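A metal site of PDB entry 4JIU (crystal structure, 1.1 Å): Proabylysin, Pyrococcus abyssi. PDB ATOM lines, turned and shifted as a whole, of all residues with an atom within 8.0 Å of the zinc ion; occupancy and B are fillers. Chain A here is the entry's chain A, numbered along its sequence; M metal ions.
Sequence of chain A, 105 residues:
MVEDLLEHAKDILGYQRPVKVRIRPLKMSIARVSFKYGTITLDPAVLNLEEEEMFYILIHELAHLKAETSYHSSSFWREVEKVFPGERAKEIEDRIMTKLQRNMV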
ATOM      1  N   ALA A  31      -7.625   0.998  -6.450  1.00  0.00           N
ATOM      2  CA  ALA A  31      -7.566   0.366  -5.136  1.00  0.00           C
ATOM      3  C   ALA A  31      -7.269  -1.096  -5.300  1.00  0.00           C
ATOM      4  O   ALA A  31      -7.726  -1.734  -6.238  1.00  0.00           O
ATOM      5  CB  ALA A  31      -8.887   0.544  -4.421  1.00  0.00           C
ATOM      6  N   ARG A  32      -6.542  -1.629  -4.303  1.00  0.00           N
ATOM      7  CA  ARG A  32      -6.276  -3.072  -4.273  1.00  0.00           C
ATOM      8  C   ARG A  32      -5.953  -3.491  -2.832  1.00  0.00           C
ATOM      9  O   ARG A  32      -5.823  -2.616  -1.989  1.00  0.00           O
ATOM     10  CB  ARG A  32      -5.128  -3.428  -5.194  1.00  0.00           C
ATOM     11  CG  ARG A  32      -3.816  -2.836  -4.690  1.00  0.00           C
ATOM     12  CD  ARG A  32      -2.655  -3.230  -5.527  1.00  0.00           C
ATOM     13  NE  ARG A  32      -1.403  -2.591  -5.151  1.00  0.00           N
ATOM     14  CZ  ARG A  32      -0.482  -2.125  -5.974  1.00  0.00           C
ATOM     15  NH1 ARG A  32      -0.587  -2.186  -7.308  1.00  0.00           N
ATOM     16  NH2 ARG A  32       0.641  -1.551  -5.559  1.00  0.00           N
ATOM     17  N   VAL A  33      -5.914  -4.773  -2.569  1.00  0.00           N
ATOM     18  CA  VAL A  33      -5.578  -5.300  -1.255  1.00  0.00           C
ATOM     19  C   VAL A  33      -4.309  -6.131  -1.305  1.00  0.00           C
ATOM     20  O   VAL A  33      -3.869  -6.643  -2.320  1.00  0.00           O
ATOM     21  CB  VAL A  33      -6.694  -6.162  -0.646  1.00  0.00           C
ATOM     22  CG1 VAL A  33      -7.974  -5.319  -0.531  1.00  0.00           C
ATOM     23  CG2 VAL A  33      -6.925  -7.460  -1.372  1.00  0.00           C
ATOM     24  N   TYR A  56     -17.922   2.708  -0.689  1.00  0.00           N
ATOM     25  CA  TYR A  56     -18.003   1.538  -1.568  1.00  0.00           C
ATOM     26  C   TYR A  56     -16.658   0.895  -1.768  1.00  0.00           C
ATOM     27  O   TYR A  56     -16.485  -0.298  -1.736  1.00  0.00           O
ATOM     28  CB  TYR A  56     -18.707   1.891  -2.922  1.00  0.00           C
ATOM     29  CG  TYR A  56     -18.676   0.670  -3.783  1.00  0.00           C
ATOM     30  CD1 TYR A  56     -19.576  -0.383  -3.518  1.00  0.00           C
ATOM     31  CD2 TYR A  56     -17.751   0.423  -4.761  1.00  0.00           C
ATOM     32  CE1 TYR A  56     -19.560  -1.515  -4.239  1.00  0.00           C
ATOM     33  CE2 TYR A  56     -17.680  -0.751  -5.453  1.00  0.00           C
ATOM     34  CZ  TYR A  56     -18.596  -1.742  -5.187  1.00  0.00           C
ATOM     35  OH  TYR A  56     -18.587  -2.930  -5.872  1.00  0.00           O
ATOM     36  N   ILE A  57     -15.650   1.722  -2.124  1.00  0.00           N
ATOM     37  CA  ILE A  57     -14.325   1.178  -2.358  1.00  0.00           C
ATOM     38  C   ILE A  57     -13.814   0.417  -1.136  1.00  0.00           C
ATOM     39  O   ILE A  57     -13.274  -0.672  -1.275  1.00  0.00           O
ATOM     40  CB  ILE A  57     -13.354   2.293  -2.818  1.00  0.00           C
ATOM     41  CG1 ILE A  57     -13.782   2.834  -4.184  1.00  0.00           C
ATOM     42  CG2 ILE A  57     -11.930   1.775  -2.812  1.00  0.00           C
ATOM     43  CD1 ILE A  57     -13.115   4.086  -4.576  1.00  0.00           C
ATOM     44  N   HIS A  60     -15.787  -2.814  -0.784  1.00  0.00           N
ATOM     45  CA  HIS A  60     -15.391  -3.738  -1.834  1.00  0.00           C
ATOM     46  C   HIS A  60     -14.076  -4.396  -1.474  1.00  0.00           C
ATOM     47  O   HIS A  60     -13.897  -5.619  -1.586  1.00  0.00           O
ATOM     48  CB  HIS A  60     -15.353  -2.976  -3.153  1.00  0.00           C
ATOM     49  CG  HIS A  60     -14.973  -3.842  -4.323  1.00  0.00           C
ATOM     50  ND1 HIS A  60     -15.881  -4.179  -5.308  1.00  0.00           N
ATOM     51  CD2 HIS A  60     -13.837  -4.446  -4.755  1.00  0.00           C
ATOM     52  CE1 HIS A  60     -15.309  -4.947  -6.236  1.00  0.00           C
ATOM     53  NE2 HIS A  60     -14.038  -5.144  -5.881  1.00  0.00           N
ATOM     54  N   GLU A  61     -13.098  -3.569  -1.105  1.00  0.00           N
ATOM     55  CA  GLU A  61     -11.779  -4.130  -0.802  1.00  0.00           C
ATOM     56  C   GLU A  61     -11.774  -4.983   0.485  1.00  0.00           C
ATOM     57  O   GLU A  61     -11.189  -6.047   0.521  1.00  0.00           O
ATOM     58  CB  GLU A  61     -10.727  -3.051  -0.779  1.00  0.00           C
ATOM     59  CG  GLU A  61     -10.571  -2.321  -2.106  1.00  0.00           C
ATOM     60  CD  GLU A  61     -10.252  -3.212  -3.277  1.00  0.00           C
ATOM     61  OE1 GLU A  61      -9.742  -4.336  -3.175  1.00  0.00           O
ATOM     62  OE2 GLU A  61     -10.546  -2.738  -4.410  1.00  0.00           O
ATOM     63  N   ALA A  63     -14.319  -6.649   1.504  1.00  0.00           N
ATOM     64  CA  ALA A  63     -15.006  -7.857   1.127  1.00  0.00           C
ATOM     65  C   ALA A  63     -14.063  -8.863   0.489  1.00  0.00           C
ATOM     66  O   ALA A  63     -14.174 -10.071   0.737  1.00  0.00           O
ATOM     67  CB  ALA A  63     -16.188  -7.550   0.206  1.00  0.00           C
ATOM     68  N   HIS A  64     -13.089  -8.400  -0.286  1.00  0.00           N
ATOM     69  CA  HIS A  64     -12.054  -9.307  -0.822  1.00  0.00           C
ATOM     70  C   HIS A  64     -11.339  -9.984   0.313  1.00  0.00           C
ATOM     71  O   HIS A  64     -11.127 -11.189   0.350  1.00  0.00           O
ATOM     72  CB  HIS A  64     -11.068  -8.561  -1.706  1.00  0.00           C
ATOM     73  CG  HIS A  64     -11.518  -8.365  -3.101  1.00  0.00           C
ATOM     74  ND1 HIS A  64     -11.794  -9.440  -3.939  1.00  0.00           N
ATOM     75  CD2 HIS A  64     -11.711  -7.238  -3.831  1.00  0.00           C
ATOM     76  CE1 HIS A  64     -12.159  -8.932  -5.116  1.00  0.00           C
ATOM     77  NE2 HIS A  64     -12.140  -7.594  -5.104  1.00  0.00           N
ATOM     78  N   THR A  69     -10.941 -13.990  -1.247  1.00  0.00           N
ATOM     79  CA  THR A  69     -10.964 -14.256  -2.687  1.00  0.00           C
ATOM     80  C   THR A  69     -10.765 -13.019  -3.526  1.00  0.00           C
ATOM     81  O   THR A  69     -11.309 -11.981  -3.138  1.00  0.00           O
ATOM     82  CB  THR A  69     -12.293 -14.945  -3.080  1.00  0.00           C
ATOM     83  OG1 THR A  69     -12.208 -15.251  -4.480  1.00  0.00           O
ATOM     84  CG2 THR A  69     -13.515 -14.109  -2.818  1.00  0.00           C
ATOM     85  N   SER A  70     -10.025 -13.161  -4.602  1.00  0.00           N
ATOM     86  CA  SER A  70      -9.937 -12.149  -5.623  1.00  0.00           C
ATOM     87  C   SER A  70     -11.055 -12.206  -6.665  1.00  0.00           C
ATOM     88  O   SER A  70     -11.323 -11.242  -7.369  1.00  0.00           O
ATOM     89  CB  SER A  70      -8.595 -12.236  -6.351  1.00  0.00           C
ATOM     90  OG  SER A  70      -7.538 -11.901  -5.503  1.00  0.00           O
ATOM     91  N   TYR A  71     -11.699 -13.358  -6.736  1.00  0.00           N
ATOM     92  CA  TYR A  71     -12.817 -13.529  -7.633  1.00  0.00           C
ATOM     93  C   TYR A  71     -14.086 -12.943  -6.992  1.00  0.00           C
ATOM     94  O   TYR A  71     -14.311 -13.166  -5.809  1.00  0.00           O
ATOM     95  CB  TYR A  71     -12.993 -15.028  -7.986  1.00  0.00           C
ATOM     96  CG  TYR A  71     -14.253 -15.271  -8.766  1.00  0.00           C
ATOM     97  CD1 TYR A  71     -15.264 -16.080  -8.251  1.00  0.00           C
ATOM     98  CD2 TYR A  71     -14.483 -14.700 -10.024  1.00  0.00           C
ATOM     99  CE1 TYR A  71     -16.416 -16.308  -8.947  1.00  0.00           C
ATOM    100  CE2 TYR A  71     -15.674 -14.928 -10.697  1.00  0.00           C
ATOM    101  CZ  TYR A  71     -16.641 -15.728 -10.135  1.00  0.00           C
ATOM    102  OH  TYR A  71     -17.830 -15.985 -10.818  1.00  0.00           O
ATOM    103  N   HIS A  72     -14.896 -12.229  -7.796  1.00  0.00           N
ATOM    104  CA  HIS A  72     -16.082 -11.616  -7.237  1.00  0.00           C
ATOM    105  C   HIS A  72     -17.210 -12.680  -7.187  1.00  0.00           C
ATOM    106  O   HIS A  72     -18.141 -12.685  -8.010  1.00  0.00           O
ATOM    107  CB  HIS A  72     -16.510 -10.430  -8.086  1.00  0.00           C
ATOM    108  CG  HIS A  72     -15.501  -9.349  -8.100  1.00  0.00           C
ATOM    109  ND1 HIS A  72     -15.202  -8.645  -9.269  1.00  0.00           N
ATOM    110  CD2 HIS A  72     -14.805  -8.704  -7.163  1.00  0.00           C
ATOM    111  CE1 HIS A  72     -14.304  -7.727  -8.947  1.00  0.00           C
ATOM    112  NE2 HIS A  72     -13.989  -7.741  -7.669  1.00  0.00           N
ATOM    113  N   PHE A  76     -18.419 -13.074  -1.904  1.00  0.00           N
ATOM    114  CA  PHE A  76     -17.912 -11.699  -1.969  1.00  0.00           C
ATOM    115  C   PHE A  76     -19.050 -10.701  -1.984  1.00  0.00           C
ATOM    116  O   PHE A  76     -19.109  -9.733  -1.235  1.00  0.00           O
ATOM    117  CB  PHE A  76     -17.008 -11.594  -3.226  1.00  0.00           C
ATOM    118  CG  PHE A  76     -16.616 -10.161  -3.512  1.00  0.00           C
ATOM    119  CD1 PHE A  76     -15.488  -9.611  -2.895  1.00  0.00           C
ATOM    120  CD2 PHE A  76     -17.349  -9.385  -4.396  1.00  0.00           C
ATOM    121  CE1 PHE A  76     -15.160  -8.296  -3.111  1.00  0.00           C
ATOM    122  CE2 PHE A  76     -17.037  -8.069  -4.579  1.00  0.00           C
ATOM    123  CZ  PHE A  76     -15.957  -7.530  -3.957  1.00  0.00           C
ATOM    124  N   TRP A  77     -19.996 -10.900  -2.915  1.00  0.00           N
ATOM    125  CA  TRP A  77     -21.074  -9.955  -3.081  1.00  0.00           C
ATOM    126  C   TRP A  77     -21.989  -9.937  -1.868  1.00  0.00           C
ATOM    127  O   TRP A  77     -22.540  -8.914  -1.529  1.00  0.00           O
ATOM    128  CB  TRP A  77     -21.881 -10.168  -4.364  1.00  0.00           C
ATOM    129  CG  TRP A  77     -21.107  -9.797  -5.569  1.00  0.00           C
ATOM    130  CD1 TRP A  77     -20.701 -10.628  -6.576  1.00  0.00           C
ATOM    131  CD2 TRP A  77     -20.587  -8.506  -5.940  1.00  0.00           C
ATOM    132  NE1 TRP A  77     -19.984  -9.988  -7.540  1.00  0.00           N
ATOM    133  CE2 TRP A  77     -19.896  -8.653  -7.160  1.00  0.00           C
ATOM    134  CE3 TRP A  77     -20.625  -7.241  -5.354  1.00  0.00           C
ATOM    135  CZ2 TRP A  77     -19.250  -7.584  -7.833  1.00  0.00           C
ATOM    136  CZ3 TRP A  77     -19.995  -6.181  -6.004  1.00  0.00           C
ATOM    137  CH2 TRP A  77     -19.320  -6.359  -7.218  1.00  0.00           C
ATOM    138  N   VAL A  80     -20.559  -7.307   0.393  1.00  0.00           N
ATOM    139  CA  VAL A  80     -20.863  -5.966  -0.149  1.00  0.00           C
ATOM    140  C   VAL A  80     -22.301  -5.571   0.105  1.00  0.00           C
ATOM    141  O   VAL A  80     -22.590  -4.412   0.473  1.00  0.00           O
ATOM    142  CB  VAL A  80     -20.513  -5.923  -1.655  1.00  0.00           C
ATOM    143  CG1 VAL A  80     -20.992  -4.635  -2.278  1.00  0.00           C
ATOM    144  CG2 VAL A  80     -19.033  -6.138  -1.899  1.00  0.00           C
ATOM    145  N   GLU A  93     -20.222   1.683  -8.661  1.00  0.00           N
ATOM    146  CA  GLU A  93     -19.092   1.426  -9.525  1.00  0.00           C
ATOM    147  C   GLU A  93     -19.142   2.232 -10.809  1.00  0.00           C
ATOM    148  O   GLU A  93     -18.119   2.757 -11.238  1.00  0.00           O
ATOM    149  CB  GLU A  93     -19.034  -0.055  -9.893  1.00  0.00           C
ATOM    150  CG  GLU A  93     -18.529  -0.926  -8.782  1.00  0.00           C
ATOM    151  CD  GLU A  93     -18.288  -2.356  -9.217  1.00  0.00           C
ATOM    152  OE1 GLU A  93     -18.106  -3.157  -8.307  1.00  0.00           O
ATOM    153  OE2 GLU A  93     -18.267  -2.753 -10.408  1.00  0.00           O
ATOM    154  N   MET A 104     -11.290  -0.335  -9.822  1.00  0.00           N
ATOM    155  CA  MET A 104     -10.694  -0.892  -8.609  1.00  0.00           C
ATOM    156  C   MET A 104     -10.502  -2.377  -8.812  1.00  0.00           C
ATOM    157  O   MET A 104     -11.335  -2.921  -9.590  1.00  0.00           O
ATOM    158  CB  MET A 104     -11.578  -0.702  -7.375  1.00  0.00           C
ATOM    159  CG  MET A 104     -12.855  -1.541  -7.299  1.00  0.00           C
ATOM    160  SD  MET A 104     -14.071  -0.778  -6.209  1.00  0.00           S
ATOM    161  CE  MET A 104     -14.641   0.542  -7.250  1.00  0.00           C
ATOM    162  N   VAL A 105      -9.579  -2.995  -8.109  1.00  0.00           N
ATOM    163  CA  VAL A 105      -9.459  -4.455  -8.206  1.00  0.00           C
ATOM    164  C   VAL A 105     -10.598  -5.071  -7.384  1.00  0.00           C
ATOM    165  O   VAL A 105     -11.326  -5.967  -7.907  1.00  0.00           O
ATOM    166  CB  VAL A 105      -8.058  -4.893  -7.726  1.00  0.00           C
ATOM    167  CG1 VAL A 105      -7.951  -6.395  -7.734  1.00  0.00           C
ATOM    168  CG2 VAL A 105      -6.976  -4.263  -8.612  1.00  0.00           C
ATOM    169  OXT VAL A 105     -10.850  -4.683  -6.235  1.00  0.00           O
HETATM  170 ZN    ZN M   1     -12.792  -6.495  -6.632  1.00  0.00          ZN
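ND1 of His 60 is in hydrogen-bond range of OH of Tyr 56 (3.0 Å). The backbone carbonyl oxygen of Thr 69 is in hydrogen-bond range of a ring nitrogen (ND1) of His 64. The chain-end carboxylate of Val 105 lies close to the side-chain carboxylate of Glu 61, at 2.7 Å. The backbone NH (N) of Val 105 sits at hydrogen-bond distance from the backbone carbonyl oxygen (O) of Ala 31 (2.9 Å). O of His 72 is in hydrogen-bond range of NE1 of Trp 77 (3.3 Å).
Within 4 Å of the zinc ion: His 60, His 64, His 72 and Val 105.
The zinc ion is bound by NE2 of His 60, 2.0 Å away. NE2 of His 64 binds the zinc ion, 2.0 Å away. O of Val 105 binds the zinc ion (2.0 Å). A ring nitrogen (NE2) of His 72 binds the zinc ion (2.0 Å). The zinc ion has four donor atoms within binding distance. Slightly farther from the zinc ion lies the chain-end carboxylate (OXT) of Val 105 (2.7 Å).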
